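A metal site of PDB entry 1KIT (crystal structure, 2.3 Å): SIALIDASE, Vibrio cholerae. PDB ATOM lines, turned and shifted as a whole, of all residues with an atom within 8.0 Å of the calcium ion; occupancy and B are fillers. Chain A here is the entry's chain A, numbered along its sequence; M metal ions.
The side-chain amide nitrogen (ND2) of Asn 232 is in hydrogen-bond range of the backbone carbonyl oxygen (O) of Asp 226 (3.0 Å). ND2 of Asn 232 sits at hydrogen-bond distance from O of Gly 225, at 3.1 Å. The backbone carbonyl oxygen of Gly 224 lies within hydrogen-bond range of the side-chain amide nitrogen of Asn 232 (3.4 Å). N of Thr 289 is in hydrogen-bond range of O of Glu 263 (2.9 Å). The side-chain carboxylate of Asp 265 lies close to the backbone NH of Gly 228, at 2.9 Å. OD1 of Asp 265 lies close to N of Asn 234. The backbone NH of Asp 265 sits at hydrogen-bond distance from the backbone carbonyl oxygen of Trp 287, at 3.0 Å.
Within 4 Å of the calcium ion: Ala 229, Asn 232, Asp 265 and Thr 289.
The calcium ion is bound by OD1 of Asn 232 (2.2 Å), OG1 of Thr 289 (2.3 Å), OD2 of Asp 265 (2.3 Å), O of Ala 229 (2.4 Å), O of Thr 289 (2.5 Å), O of Asn 232 (2.5 Å) and OD1 of Asp 265 (2.8 Å).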
ATOM      1  N   VAL A 222      18.108 -21.557 -30.654  1.00  0.00           N
ATOM      2  CA  VAL A 222      17.157 -20.498 -30.351  1.00  0.00           C
ATOM      3  C   VAL A 222      17.586 -19.784 -29.065  1.00  0.00           C
ATOM      4  O   VAL A 222      17.382 -20.274 -27.925  1.00  0.00           O
ATOM      5  CB  VAL A 222      15.709 -21.056 -30.252  1.00  0.00           C
ATOM      6  CG1 VAL A 222      14.721 -19.932 -30.068  1.00  0.00           C
ATOM      7  CG2 VAL A 222      15.370 -21.839 -31.513  1.00  0.00           C
ATOM      8  N   GLY A 224      20.722 -18.426 -29.344  1.00  0.00           N
ATOM      9  CA  GLY A 224      22.127 -18.376 -29.742  1.00  0.00           C
ATOM     10  C   GLY A 224      22.934 -18.951 -28.598  1.00  0.00           C
ATOM     11  O   GLY A 224      22.405 -19.117 -27.513  1.00  0.00           O
ATOM     12  N   GLY A 225      24.198 -19.290 -28.838  1.00  0.00           N
ATOM     13  CA  GLY A 225      25.055 -19.811 -27.750  1.00  0.00           C
ATOM     14  C   GLY A 225      25.149 -21.361 -27.596  1.00  0.00           C
ATOM     15  O   GLY A 225      24.224 -22.117 -27.977  1.00  0.00           O
ATOM     16  N   ASP A 226      26.262 -21.796 -27.032  1.00  0.00           N
ATOM     17  CA  ASP A 226      26.530 -23.208 -26.762  1.00  0.00           C
ATOM     18  C   ASP A 226      25.513 -23.810 -25.830  1.00  0.00           C
ATOM     19  O   ASP A 226      24.929 -23.146 -24.998  1.00  0.00           O
ATOM     20  CB  ASP A 226      27.900 -23.368 -26.088  1.00  0.00           C
ATOM     21  CG  ASP A 226      29.023 -22.898 -26.959  1.00  0.00           C
ATOM     22  OD1 ASP A 226      28.882 -23.021 -28.209  1.00  0.00           O
ATOM     23  OD2 ASP A 226      30.025 -22.413 -26.403  1.00  0.00           O
ATOM     24  N   PRO A 227      25.313 -25.110 -25.996  1.00  0.00           N
ATOM     25  CA  PRO A 227      24.394 -25.844 -25.169  1.00  0.00           C
ATOM     26  C   PRO A 227      24.741 -25.621 -23.694  1.00  0.00           C
ATOM     27  O   PRO A 227      25.890 -25.361 -23.363  1.00  0.00           O
ATOM     28  CB  PRO A 227      24.632 -27.306 -25.574  1.00  0.00           C
ATOM     29  CG  PRO A 227      25.845 -27.332 -26.325  1.00  0.00           C
ATOM     30  CD  PRO A 227      26.091 -25.970 -26.896  1.00  0.00           C
ATOM     31  N   GLY A 228      23.727 -25.655 -22.840  1.00  0.00           N
ATOM     32  CA  GLY A 228      23.912 -25.461 -21.415  1.00  0.00           C
ATOM     33  C   GLY A 228      23.437 -24.104 -20.971  1.00  0.00           C
ATOM     34  O   GLY A 228      23.257 -23.880 -19.796  1.00  0.00           O
ATOM     35  N   ALA A 229      23.139 -23.197 -21.912  1.00  0.00           N
ATOM     36  CA  ALA A 229      22.619 -21.881 -21.496  1.00  0.00           C
ATOM     37  C   ALA A 229      21.190 -21.914 -21.085  1.00  0.00           C
ATOM     38  O   ALA A 229      20.328 -22.425 -21.778  1.00  0.00           O
ATOM     39  CB  ALA A 229      22.849 -20.775 -22.544  1.00  0.00           C
ATOM     40  N   LEU A 230      20.923 -21.351 -19.931  1.00  0.00           N
ATOM     41  CA  LEU A 230      19.573 -21.253 -19.471  1.00  0.00           C
ATOM     42  C   LEU A 230      18.815 -20.427 -20.507  1.00  0.00           C
ATOM     43  O   LEU A 230      17.590 -20.422 -20.546  1.00  0.00           O
ATOM     44  CB  LEU A 230      19.563 -20.493 -18.175  1.00  0.00           C
ATOM     45  CG  LEU A 230      18.248 -20.599 -17.443  1.00  0.00           C
ATOM     46  CD1 LEU A 230      18.251 -21.823 -16.507  1.00  0.00           C
ATOM     47  CD2 LEU A 230      17.995 -19.330 -16.703  1.00  0.00           C
ATOM     48  N   SER A 231      19.576 -19.674 -21.296  1.00  0.00           N
ATOM     49  CA  SER A 231      19.003 -18.773 -22.281  1.00  0.00           C
ATOM     50  C   SER A 231      19.077 -19.318 -23.691  1.00  0.00           C
ATOM     51  O   SER A 231      19.494 -18.631 -24.598  1.00  0.00           O
ATOM     52  CB  SER A 231      19.674 -17.413 -22.211  1.00  0.00           C
ATOM     53  OG  SER A 231      21.020 -17.504 -22.655  1.00  0.00           O
ATOM     54  N   ASN A 232      18.649 -20.559 -23.884  1.00  0.00           N
ATOM     55  CA  ASN A 232      18.586 -21.140 -25.218  1.00  0.00           C
ATOM     56  C   ASN A 232      17.943 -22.485 -25.198  1.00  0.00           C
ATOM     57  O   ASN A 232      17.724 -23.063 -24.149  1.00  0.00           O
ATOM     58  CB  ASN A 232      19.958 -21.149 -25.947  1.00  0.00           C
ATOM     59  CG  ASN A 232      20.967 -22.193 -25.362  1.00  0.00           C
ATOM     60  OD1 ASN A 232      20.576 -23.210 -24.795  1.00  0.00           O
ATOM     61  ND2 ASN A 232      22.258 -21.936 -25.551  1.00  0.00           N
ATOM     62  N   THR A 233      17.653 -22.988 -26.373  1.00  0.00           N
ATOM     63  CA  THR A 233      17.113 -24.318 -26.531  1.00  0.00           C
ATOM     64  C   THR A 233      17.694 -24.666 -27.841  1.00  0.00           C
ATOM     65  O   THR A 233      17.481 -23.956 -28.845  1.00  0.00           O
ATOM     66  CB  THR A 233      15.597 -24.321 -26.655  1.00  0.00           C
ATOM     67  OG1 THR A 233      15.020 -23.780 -25.452  1.00  0.00           O
ATOM     68  CG2 THR A 233      15.112 -25.753 -26.882  1.00  0.00           C
ATOM     69  N   ASN A 234      18.584 -25.652 -27.839  1.00  0.00           N
ATOM     70  CA  ASN A 234      19.233 -26.003 -29.056  1.00  0.00           C
ATOM     71  C   ASN A 234      18.688 -27.292 -29.575  1.00  0.00           C
ATOM     72  O   ASN A 234      18.386 -28.194 -28.780  1.00  0.00           O
ATOM     73  CB  ASN A 234      20.743 -26.014 -28.880  1.00  0.00           C
ATOM     74  CG  ASN A 234      21.269 -24.644 -28.444  1.00  0.00           C
ATOM     75  OD1 ASN A 234      20.531 -23.680 -28.439  1.00  0.00           O
ATOM     76  ND2 ASN A 234      22.570 -24.563 -28.073  1.00  0.00           N
ATOM     77  N   ASN A 259      12.184 -33.121 -27.745  1.00  0.00           N
ATOM     78  CA  ASN A 259      12.253 -32.156 -26.660  1.00  0.00           C
ATOM     79  C   ASN A 259      10.948 -31.376 -26.543  1.00  0.00           C
ATOM     80  O   ASN A 259      10.858 -30.194 -26.926  1.00  0.00           O
ATOM     81  CB  ASN A 259      13.467 -31.262 -26.900  1.00  0.00           C
ATOM     82  CG  ASN A 259      13.800 -30.347 -25.726  1.00  0.00           C
ATOM     83  OD1 ASN A 259      13.329 -30.545 -24.580  1.00  0.00           O
ATOM     84  ND2 ASN A 259      14.632 -29.362 -25.961  1.00  0.00           N
ATOM     85  N   ASP A 262      11.179 -28.415 -24.252  1.00  0.00           N
ATOM     86  CA  ASP A 262      12.418 -27.703 -24.521  1.00  0.00           C
ATOM     87  C   ASP A 262      13.251 -27.709 -23.283  1.00  0.00           C
ATOM     88  O   ASP A 262      13.971 -26.765 -22.970  1.00  0.00           O
ATOM     89  CB  ASP A 262      12.091 -26.266 -24.933  1.00  0.00           C
ATOM     90  CG  ASP A 262      11.052 -26.212 -26.053  1.00  0.00           C
ATOM     91  OD1 ASP A 262      10.805 -27.240 -26.716  1.00  0.00           O
ATOM     92  OD2 ASP A 262      10.398 -25.142 -26.169  1.00  0.00           O
ATOM     93  N   GLU A 263      13.193 -28.868 -22.639  1.00  0.00           N
ATOM     94  CA  GLU A 263      13.900 -29.137 -21.438  1.00  0.00           C
ATOM     95  C   GLU A 263      15.334 -29.526 -21.777  1.00  0.00           C
ATOM     96  O   GLU A 263      16.204 -29.512 -20.887  1.00  0.00           O
ATOM     97  CB  GLU A 263      13.204 -30.288 -20.727  1.00  0.00           C
ATOM     98  CG  GLU A 263      13.711 -30.567 -19.377  1.00  0.00           C
ATOM     99  CD  GLU A 263      13.034 -31.755 -18.787  1.00  0.00           C
ATOM    100  OE1 GLU A 263      12.078 -32.277 -19.428  1.00  0.00           O
ATOM    101  OE2 GLU A 263      13.419 -32.195 -17.689  1.00  0.00           O
ATOM    102  N   PHE A 264      15.623 -29.819 -23.021  1.00  0.00           N
ATOM    103  CA  PHE A 264      16.950 -30.216 -23.369  1.00  0.00           C
ATOM    104  C   PHE A 264      17.622 -29.301 -24.367  1.00  0.00           C
ATOM    105  O   PHE A 264      17.054 -28.328 -24.851  1.00  0.00           O
ATOM    106  CB  PHE A 264      16.965 -31.667 -23.869  1.00  0.00           C
ATOM    107  CG  PHE A 264      16.287 -32.641 -22.929  1.00  0.00           C
ATOM    108  CD1 PHE A 264      16.878 -32.991 -21.710  1.00  0.00           C
ATOM    109  CD2 PHE A 264      15.071 -33.217 -23.279  1.00  0.00           C
ATOM    110  CE1 PHE A 264      16.270 -33.923 -20.848  1.00  0.00           C
ATOM    111  CE2 PHE A 264      14.420 -34.123 -22.406  1.00  0.00           C
ATOM    112  CZ  PHE A 264      15.012 -34.461 -21.193  1.00  0.00           C
ATOM    113  N   ASP A 265      18.868 -29.588 -24.636  1.00  0.00           N
ATOM    114  CA  ASP A 265      19.618 -28.883 -25.644  1.00  0.00           C
ATOM    115  C   ASP A 265      20.233 -30.040 -26.396  1.00  0.00           C
ATOM    116  O   ASP A 265      20.611 -31.046 -25.776  1.00  0.00           O
ATOM    117  CB  ASP A 265      20.743 -28.044 -25.011  1.00  0.00           C
ATOM    118  CG  ASP A 265      20.334 -26.600 -24.748  1.00  0.00           C
ATOM    119  OD1 ASP A 265      19.263 -26.159 -25.209  1.00  0.00           O
ATOM    120  OD2 ASP A 265      21.094 -25.882 -24.073  1.00  0.00           O
ATOM    121  N   PHE A 266      20.260 -29.981 -27.722  1.00  0.00           N
ATOM    122  CA  PHE A 266      20.925 -31.043 -28.446  1.00  0.00           C
ATOM    123  C   PHE A 266      22.136 -30.459 -29.121  1.00  0.00           C
ATOM    124  O   PHE A 266      22.212 -29.248 -29.355  1.00  0.00           O
ATOM    125  CB  PHE A 266      19.997 -31.768 -29.405  1.00  0.00           C
ATOM    126  CG  PHE A 266      18.830 -32.408 -28.720  1.00  0.00           C
ATOM    127  CD1 PHE A 266      17.750 -31.657 -28.315  1.00  0.00           C
ATOM    128  CD2 PHE A 266      18.874 -33.758 -28.387  1.00  0.00           C
ATOM    129  CE1 PHE A 266      16.669 -32.266 -27.661  1.00  0.00           C
ATOM    130  CE2 PHE A 266      17.861 -34.360 -27.703  1.00  0.00           C
ATOM    131  CZ  PHE A 266      16.721 -33.638 -27.374  1.00  0.00           C
ATOM    132  N   TRP A 287      21.691 -32.716 -23.498  1.00  0.00           N
ATOM    133  CA  TRP A 287      22.119 -32.146 -22.219  1.00  0.00           C
ATOM    134  C   TRP A 287      20.833 -31.509 -21.687  1.00  0.00           C
ATOM    135  O   TRP A 287      19.895 -31.307 -22.455  1.00  0.00           O
ATOM    136  CB  TRP A 287      23.158 -31.024 -22.482  1.00  0.00           C
ATOM    137  CG  TRP A 287      24.215 -31.370 -23.511  1.00  0.00           C
ATOM    138  CD1 TRP A 287      24.116 -31.232 -24.849  1.00  0.00           C
ATOM    139  CD2 TRP A 287      25.520 -31.907 -23.264  1.00  0.00           C
ATOM    140  NE1 TRP A 287      25.257 -31.660 -25.454  1.00  0.00           N
ATOM    141  CE2 TRP A 287      26.135 -32.110 -24.509  1.00  0.00           C
ATOM    142  CE3 TRP A 287      26.231 -32.253 -22.109  1.00  0.00           C
ATOM    143  CZ2 TRP A 287      27.412 -32.659 -24.642  1.00  0.00           C
ATOM    144  CZ3 TRP A 287      27.518 -32.772 -22.241  1.00  0.00           C
ATOM    145  CH2 TRP A 287      28.094 -32.977 -23.500  1.00  0.00           C
ATOM    146  N   PRO A 288      20.790 -31.168 -20.418  1.00  0.00           N
ATOM    147  CA  PRO A 288      19.608 -30.443 -19.943  1.00  0.00           C
ATOM    148  C   PRO A 288      19.836 -29.042 -20.503  1.00  0.00           C
ATOM    149  O   PRO A 288      20.987 -28.671 -20.796  1.00  0.00           O
ATOM    150  CB  PRO A 288      19.785 -30.401 -18.424  1.00  0.00           C
ATOM    151  CG  PRO A 288      21.267 -30.578 -18.223  1.00  0.00           C
ATOM    152  CD  PRO A 288      21.669 -31.557 -19.314  1.00  0.00           C
ATOM    153  N   THR A 289      18.775 -28.273 -20.667  1.00  0.00           N
ATOM    154  CA  THR A 289      18.932 -26.954 -21.233  1.00  0.00           C
ATOM    155  C   THR A 289      19.845 -26.048 -20.392  1.00  0.00           C
ATOM    156  O   THR A 289      20.385 -25.090 -20.900  1.00  0.00           O
ATOM    157  CB  THR A 289      17.583 -26.292 -21.459  1.00  0.00           C
ATOM    158  OG1 THR A 289      17.752 -25.137 -22.301  1.00  0.00           O
ATOM    159  CG2 THR A 289      16.959 -25.868 -20.116  1.00  0.00           C
ATOM    160  N   ASP A 290      20.061 -26.369 -19.130  1.00  0.00           N
ATOM    161  CA  ASP A 290      20.880 -25.498 -18.303  1.00  0.00           C
ATOM    162  C   ASP A 290      22.297 -25.932 -17.962  1.00  0.00           C
ATOM    163  O   ASP A 290      22.994 -25.225 -17.241  1.00  0.00           O
ATOM    164  CB  ASP A 290      20.131 -25.082 -17.021  1.00  0.00           C
ATOM    165  CG  ASP A 290      19.717 -26.267 -16.185  1.00  0.00           C
ATOM    166  OD1 ASP A 290      19.898 -27.398 -16.700  1.00  0.00           O
ATOM    167  OD2 ASP A 290      19.238 -26.078 -15.037  1.00  0.00           O
ATOM    168  N   ALA A 291      22.718 -27.111 -18.393  1.00  0.00           N
ATOM    169  CA  ALA A 291      24.082 -27.536 -18.079  1.00  0.00           C
ATOM    170  C   ALA A 291      24.601 -28.506 -19.106  1.00  0.00           C
ATOM    171  O   ALA A 291      23.850 -29.328 -19.649  1.00  0.00           O
ATOM    172  CB  ALA A 291      24.177 -28.130 -16.692  1.00  0.00           C
HETATM  173 CA    CA M   1      19.665 -24.297 -23.137  1.00  0.00          CA
